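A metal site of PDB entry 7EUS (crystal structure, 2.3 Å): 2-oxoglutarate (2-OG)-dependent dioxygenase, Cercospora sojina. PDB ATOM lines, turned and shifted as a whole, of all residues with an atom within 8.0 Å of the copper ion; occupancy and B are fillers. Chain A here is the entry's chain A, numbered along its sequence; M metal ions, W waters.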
ATOM      1  N   LEU A 138     -27.477   5.385  21.235  1.00  0.00           N
ATOM      2  CA  LEU A 138     -26.059   5.005  21.275  1.00  0.00           C
ATOM      3  C   LEU A 138     -25.697   4.712  22.734  1.00  0.00           C
ATOM      4  O   LEU A 138     -25.978   5.596  23.600  1.00  0.00           O
ATOM      5  CB  LEU A 138     -25.238   6.144  20.684  1.00  0.00           C
ATOM      6  CG  LEU A 138     -23.728   5.924  20.743  1.00  0.00           C
ATOM      7  CD1 LEU A 138     -23.317   4.795  19.801  1.00  0.00           C
ATOM      8  CD2 LEU A 138     -22.985   7.212  20.429  1.00  0.00           C
ATOM      9  N   ARG A 140     -22.665   4.337  25.376  1.00  0.00           N
ATOM     10  CA  ARG A 140     -21.280   4.760  25.726  1.00  0.00           C
ATOM     11  C   ARG A 140     -20.868   3.990  26.994  1.00  0.00           C
ATOM     12  O   ARG A 140     -21.667   3.970  27.941  1.00  0.00           O
ATOM     13  CB  ARG A 140     -21.205   6.276  25.943  1.00  0.00           C
ATOM     14  CG  ARG A 140     -21.454   7.095  24.688  1.00  0.00           C
ATOM     15  CD  ARG A 140     -21.308   8.597  24.868  1.00  0.00           C
ATOM     16  NE  ARG A 140     -21.608   9.163  23.593  1.00  0.00           N
ATOM     17  CZ  ARG A 140     -20.793   9.296  22.542  1.00  0.00           C
ATOM     18  NH1 ARG A 140     -19.558   8.844  22.513  1.00  0.00           N
ATOM     19  NH2 ARG A 140     -21.284   9.941  21.498  1.00  0.00           N
ATOM     20  N   GLY A 166     -17.974  11.343  23.973  1.00  0.00           N
ATOM     21  CA  GLY A 166     -17.920  12.352  22.906  1.00  0.00           C
ATOM     22  C   GLY A 166     -17.170  13.580  23.362  1.00  0.00           C
ATOM     23  O   GLY A 166     -17.810  14.592  23.633  1.00  0.00           O
ATOM     24  N   PHE A 168     -15.555  16.182  22.157  1.00  0.00           N
ATOM     25  CA  PHE A 168     -15.382  17.338  21.241  1.00  0.00           C
ATOM     26  C   PHE A 168     -16.716  18.085  21.155  1.00  0.00           C
ATOM     27  O   PHE A 168     -17.828  17.518  21.352  1.00  0.00           O
ATOM     28  CB  PHE A 168     -14.877  16.873  19.864  1.00  0.00           C
ATOM     29  CG  PHE A 168     -15.818  15.918  19.178  1.00  0.00           C
ATOM     30  CD1 PHE A 168     -15.870  14.579  19.558  1.00  0.00           C
ATOM     31  CD2 PHE A 168     -16.671  16.340  18.180  1.00  0.00           C
ATOM     32  CE1 PHE A 168     -16.743  13.694  18.948  1.00  0.00           C
ATOM     33  CE2 PHE A 168     -17.554  15.463  17.562  1.00  0.00           C
ATOM     34  CZ  PHE A 168     -17.567  14.129  17.926  1.00  0.00           C
ATOM     35  N   VAL A 169     -16.622  19.358  20.843  1.00  0.00           N
ATOM     36  CA  VAL A 169     -17.783  20.273  20.904  1.00  0.00           C
ATOM     37  C   VAL A 169     -18.513  20.118  19.581  1.00  0.00           C
ATOM     38  O   VAL A 169     -17.911  20.387  18.522  1.00  0.00           O
ATOM     39  CB  VAL A 169     -17.335  21.723  21.116  1.00  0.00           C
ATOM     40  CG1 VAL A 169     -18.498  22.685  21.010  1.00  0.00           C
ATOM     41  CG2 VAL A 169     -16.618  21.851  22.441  1.00  0.00           C
ATOM     42  N   HIS A 170     -19.772  19.726  19.618  1.00  0.00           N
ATOM     43  CA  HIS A 170     -20.532  19.490  18.365  1.00  0.00           C
ATOM     44  C   HIS A 170     -22.005  19.657  18.670  1.00  0.00           C
ATOM     45  O   HIS A 170     -22.389  19.546  19.822  1.00  0.00           O
ATOM     46  CB  HIS A 170     -20.224  18.080  17.838  1.00  0.00           C
ATOM     47  CG  HIS A 170     -20.620  17.037  18.842  1.00  0.00           C
ATOM     48  ND1 HIS A 170     -19.841  16.710  19.903  1.00  0.00           N
ATOM     49  CD2 HIS A 170     -21.752  16.319  18.979  1.00  0.00           C
ATOM     50  CE1 HIS A 170     -20.464  15.832  20.657  1.00  0.00           C
ATOM     51  NE2 HIS A 170     -21.651  15.554  20.107  1.00  0.00           N
ATOM     52  N   VAL A 171     -22.804  19.771  17.634  1.00  0.00           N
ATOM     53  CA  VAL A 171     -24.256  19.445  17.685  1.00  0.00           C
ATOM     54  C   VAL A 171     -24.425  18.298  16.710  1.00  0.00           C
ATOM     55  O   VAL A 171     -23.800  18.364  15.618  1.00  0.00           O
ATOM     56  CB  VAL A 171     -25.071  20.679  17.302  1.00  0.00           C
ATOM     57  CG1 VAL A 171     -26.546  20.456  17.537  1.00  0.00           C
ATOM     58  CG2 VAL A 171     -24.581  21.891  18.054  1.00  0.00           C
ATOM     59  N   ASP A 172     -25.259  17.316  17.062  1.00  0.00           N
ATOM     60  CA  ASP A 172     -25.402  16.039  16.324  1.00  0.00           C
ATOM     61  C   ASP A 172     -25.904  16.298  14.908  1.00  0.00           C
ATOM     62  O   ASP A 172     -25.512  15.534  13.993  1.00  0.00           O
ATOM     63  CB  ASP A 172     -26.338  15.098  17.087  1.00  0.00           C
ATOM     64  CG  ASP A 172     -25.757  14.619  18.411  1.00  0.00           C
ATOM     65  OD1 ASP A 172     -24.664  15.091  18.810  1.00  0.00           O
ATOM     66  OD2 ASP A 172     -26.410  13.786  19.031  1.00  0.00           O
ATOM     67  N   GLN A 173     -26.760  17.304  14.740  1.00  0.00           N
ATOM     68  CA  GLN A 173     -27.330  17.699  13.435  1.00  0.00           C
ATOM     69  C   GLN A 173     -27.137  19.202  13.226  1.00  0.00           C
ATOM     70  O   GLN A 173     -27.445  19.986  14.139  1.00  0.00           O
ATOM     71  CB  GLN A 173     -28.792  17.267  13.325  1.00  0.00           C
ATOM     72  CG  GLN A 173     -28.984  15.762  13.103  1.00  0.00           C
ATOM     73  CD  GLN A 173     -28.861  14.949  14.371  1.00  0.00           C
ATOM     74  OE1 GLN A 173     -29.270  15.383  15.439  1.00  0.00           O
ATOM     75  NE2 GLN A 173     -28.294  13.747  14.244  1.00  0.00           N
ATOM     76  N   ASN A 203     -32.203  14.916  21.967  1.00  0.00           N
ATOM     77  CA  ASN A 203     -31.507  13.757  22.569  1.00  0.00           C
ATOM     78  C   ASN A 203     -31.865  13.667  24.044  1.00  0.00           C
ATOM     79  O   ASN A 203     -31.888  14.720  24.701  1.00  0.00           O
ATOM     80  CB  ASN A 203     -29.987  13.827  22.426  1.00  0.00           C
ATOM     81  CG  ASN A 203     -29.454  13.102  21.196  1.00  0.00           C
ATOM     82  OD1 ASN A 203     -30.135  13.001  20.175  1.00  0.00           O
ATOM     83  ND2 ASN A 203     -28.224  12.626  21.285  1.00  0.00           N
ATOM     84  N   TRP A 205     -30.386  11.902  27.314  1.00  0.00           N
ATOM     85  CA  TRP A 205     -29.106  11.372  27.834  1.00  0.00           C
ATOM     86  C   TRP A 205     -29.325  10.889  29.264  1.00  0.00           C
ATOM     87  O   TRP A 205     -29.805  11.673  30.076  1.00  0.00           O
ATOM     88  CB  TRP A 205     -28.012  12.436  27.741  1.00  0.00           C
ATOM     89  CG  TRP A 205     -26.620  11.934  27.955  1.00  0.00           C
ATOM     90  CD1 TRP A 205     -25.740  11.535  26.995  1.00  0.00           C
ATOM     91  CD2 TRP A 205     -25.939  11.787  29.215  1.00  0.00           C
ATOM     92  NE1 TRP A 205     -24.554  11.159  27.568  1.00  0.00           N
ATOM     93  CE2 TRP A 205     -24.641  11.309  28.924  1.00  0.00           C
ATOM     94  CE3 TRP A 205     -26.290  12.023  30.557  1.00  0.00           C
ATOM     95  CZ2 TRP A 205     -23.703  11.035  29.925  1.00  0.00           C
ATOM     96  CZ3 TRP A 205     -25.357  11.792  31.543  1.00  0.00           C
ATOM     97  CH2 TRP A 205     -24.075  11.310  31.227  1.00  0.00           C
ATOM     98  N   LEU A 216     -21.161  14.926  31.150  1.00  0.00           N
ATOM     99  CA  LEU A 216     -21.537  15.592  29.886  1.00  0.00           C
ATOM    100  C   LEU A 216     -21.847  17.070  30.121  1.00  0.00           C
ATOM    101  O   LEU A 216     -22.694  17.363  30.976  1.00  0.00           O
ATOM    102  CB  LEU A 216     -22.745  14.906  29.269  1.00  0.00           C
ATOM    103  CG  LEU A 216     -23.147  15.443  27.898  1.00  0.00           C
ATOM    104  CD1 LEU A 216     -22.083  15.121  26.857  1.00  0.00           C
ATOM    105  CD2 LEU A 216     -24.471  14.856  27.482  1.00  0.00           C
ATOM    106  N   HIS A 234     -20.001  13.924   9.484  1.00  0.00           N
ATOM    107  CA  HIS A 234     -19.734  12.829  10.451  1.00  0.00           C
ATOM    108  C   HIS A 234     -19.959  11.498   9.730  1.00  0.00           C
ATOM    109  O   HIS A 234     -21.060  11.286   9.157  1.00  0.00           O
ATOM    110  CB  HIS A 234     -20.656  13.062  11.640  1.00  0.00           C
ATOM    111  CG  HIS A 234     -20.506  12.053  12.712  1.00  0.00           C
ATOM    112  ND1 HIS A 234     -21.181  10.855  12.680  1.00  0.00           N
ATOM    113  CD2 HIS A 234     -19.769  12.068  13.844  1.00  0.00           C
ATOM    114  CE1 HIS A 234     -20.864  10.155  13.744  1.00  0.00           C
ATOM    115  NE2 HIS A 234     -20.003  10.884  14.474  1.00  0.00           N
ATOM    116  N   MET A 250     -23.130  17.354  11.033  1.00  0.00           N
ATOM    117  CA  MET A 250     -23.220  17.924  12.347  1.00  0.00           C
ATOM    118  C   MET A 250     -22.712  19.357  12.297  1.00  0.00           C
ATOM    119  O   MET A 250     -22.338  19.841  11.240  1.00  0.00           O
ATOM    120  CB  MET A 250     -22.533  17.002  13.348  1.00  0.00           C
ATOM    121  CG  MET A 250     -21.017  17.016  13.341  1.00  0.00           C
ATOM    122  SD  MET A 250     -20.486  15.633  14.638  1.00  0.00           S
ATOM    123  CE  MET A 250     -22.015  14.538  15.066  1.00  0.00           C
ATOM    124  N   ILE A 278     -31.485  17.335  25.430  1.00  0.00           N
ATOM    125  CA  ILE A 278     -30.616  18.264  24.643  1.00  0.00           C
ATOM    126  C   ILE A 278     -31.260  18.487  23.283  1.00  0.00           C
ATOM    127  O   ILE A 278     -31.364  17.527  22.515  1.00  0.00           O
ATOM    128  CB  ILE A 278     -29.193  17.712  24.486  1.00  0.00           C
ATOM    129  CG1 ILE A 278     -28.607  17.235  25.817  1.00  0.00           C
ATOM    130  CG2 ILE A 278     -28.314  18.732  23.799  1.00  0.00           C
ATOM    131  CD1 ILE A 278     -27.374  16.406  25.691  1.00  0.00           C
ATOM    132  N   MET A 280     -30.892  19.247  19.730  1.00  0.00           N
ATOM    133  CA  MET A 280     -30.008  19.296  18.582  1.00  0.00           C
ATOM    134  C   MET A 280     -30.517  20.240  17.478  1.00  0.00           C
ATOM    135  O   MET A 280     -29.737  20.845  16.719  1.00  0.00           O
ATOM    136  CB  MET A 280     -29.900  17.871  18.013  1.00  0.00           C
ATOM    137  CG  MET A 280     -29.244  16.872  18.913  1.00  0.00           C
ATOM    138  SD  MET A 280     -27.710  17.598  19.922  1.00  0.00           S
ATOM    139  CE  MET A 280     -27.405  16.113  21.198  1.00  0.00           C
ATOM    140  N   VAL A 292     -27.805  22.926  20.569  1.00  0.00           N
ATOM    141  CA  VAL A 292     -26.975  23.019  21.796  1.00  0.00           C
ATOM    142  C   VAL A 292     -25.648  22.300  21.561  1.00  0.00           C
ATOM    143  O   VAL A 292     -25.610  21.068  21.391  1.00  0.00           O
ATOM    144  CB  VAL A 292     -27.740  22.453  22.994  1.00  0.00           C
ATOM    145  CG1 VAL A 292     -26.844  22.263  24.196  1.00  0.00           C
ATOM    146  CG2 VAL A 292     -28.966  23.320  23.306  1.00  0.00           C
ATOM    147  N   PRO A 293     -24.531  23.058  21.514  1.00  0.00           N
ATOM    148  CA  PRO A 293     -23.201  22.458  21.505  1.00  0.00           C
ATOM    149  C   PRO A 293     -23.015  21.686  22.808  1.00  0.00           C
ATOM    150  O   PRO A 293     -23.330  22.244  23.826  1.00  0.00           O
ATOM    151  CB  PRO A 293     -22.261  23.684  21.358  1.00  0.00           C
ATOM    152  CG  PRO A 293     -23.140  24.670  20.630  1.00  0.00           C
ATOM    153  CD  PRO A 293     -24.486  24.506  21.307  1.00  0.00           C
ATOM    154  N   HIS A 294     -22.610  20.420  22.731  1.00  0.00           N
ATOM    155  CA  HIS A 294     -22.373  19.530  23.895  1.00  0.00           C
ATOM    156  C   HIS A 294     -20.992  18.876  23.747  1.00  0.00           C
ATOM    157  O   HIS A 294     -20.513  18.732  22.608  1.00  0.00           O
ATOM    158  CB  HIS A 294     -23.545  18.549  24.054  1.00  0.00           C
ATOM    159  CG  HIS A 294     -23.843  17.673  22.878  1.00  0.00           C
ATOM    160  ND1 HIS A 294     -24.464  18.150  21.744  1.00  0.00           N
ATOM    161  CD2 HIS A 294     -23.579  16.369  22.648  1.00  0.00           C
ATOM    162  CE1 HIS A 294     -24.585  17.162  20.869  1.00  0.00           C
ATOM    163  NE2 HIS A 294     -24.068  16.050  21.403  1.00  0.00           N
ATOM    164  N   SER A 295     -20.423  18.424  24.864  1.00  0.00           N
ATOM    165  CA  SER A 295     -19.098  17.749  24.944  1.00  0.00           C
ATOM    166  C   SER A 295     -18.987  17.021  26.281  1.00  0.00           C
ATOM    167  O   SER A 295     -19.379  17.604  27.299  1.00  0.00           O
ATOM    168  CB  SER A 295     -17.946  18.709  24.816  1.00  0.00           C
ATOM    169  OG  SER A 295     -16.723  17.990  24.740  1.00  0.00           O
ATOM    170  N   SER A 296     -18.406  15.815  26.256  1.00  0.00           N
ATOM    171  CA  SER A 296     -17.936  15.154  27.489  1.00  0.00           C
ATOM    172  C   SER A 296     -16.723  15.937  28.012  1.00  0.00           C
ATOM    173  O   SER A 296     -16.100  16.671  27.195  1.00  0.00           O
ATOM    174  CB  SER A 296     -17.638  13.684  27.225  1.00  0.00           C
ATOM    175  OG  SER A 296     -16.383  13.522  26.592  1.00  0.00           O
ATOM    176  N   GLU A 311     -27.775   7.700  24.900  1.00  0.00           N
ATOM    177  CA  GLU A 311     -28.377   8.924  24.320  1.00  0.00           C
ATOM    178  C   GLU A 311     -29.410   8.435  23.314  1.00  0.00           C
ATOM    179  O   GLU A 311     -28.994   7.643  22.449  1.00  0.00           O
ATOM    180  CB  GLU A 311     -27.324   9.748  23.555  1.00  0.00           C
ATOM    181  CG  GLU A 311     -25.990   9.102  23.698  1.00  0.00           C
ATOM    182  CD  GLU A 311     -24.766   9.743  23.152  1.00  0.00           C
ATOM    183  OE1 GLU A 311     -23.761   9.683  23.861  1.00  0.00           O
ATOM    184  OE2 GLU A 311     -24.790  10.234  22.052  1.00  0.00           O
HETATM  185 CU    CU M   1     -23.498  14.365  20.626  1.00  0.00          CU
HETATM  186  O   HOH W   1     -22.809  12.640  19.254  1.00  0.00           O
HETATM  187  O   HOH W   2     -23.008  12.893  23.618  1.00  0.00           O
HETATM  188  O   HOH W   3     -25.441  13.400  22.359  1.00  0.00           O
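The side-chain carboxylate (OD2) of Asp 172 lies within hydrogen-bond range of the side-chain amide nitrogen (ND2) of Asn 203 (3.1 Å). The side-chain sulfur (SD) of Met 280 sits close to a ring nitrogen (ND1) of His 294 (3.8 Å). O of Val 292 lies within hydrogen-bond range of ND1 of His 294, 3.2 Å away. The backbone NH of Asp 172 lies within hydrogen-bond range of the side-chain sulfur of Met 280, at 3.8 Å. ND1 of His 170 sits at hydrogen-bond distance from O of Phe 168 (2.6 Å).
Of the 22 residues printed, 3 come within 4 Å of the copper ion. The nearest printed residue that does not touch the copper ion is Met 280 (4.3 Å).
The copper ion is bound by a ring nitrogen (NE2) of His 294, a ring nitrogen (NE2) of His 170, the side-chain carboxylate (OD1) of Asp 172 and water W1. Slightly farther from the copper ion lies water W3 (2.8 Å).
Water W3 lies within hydrogen-bond range of ND2 of Asn 203, OE2 of Glu 311 and OD2 of Asp 172.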
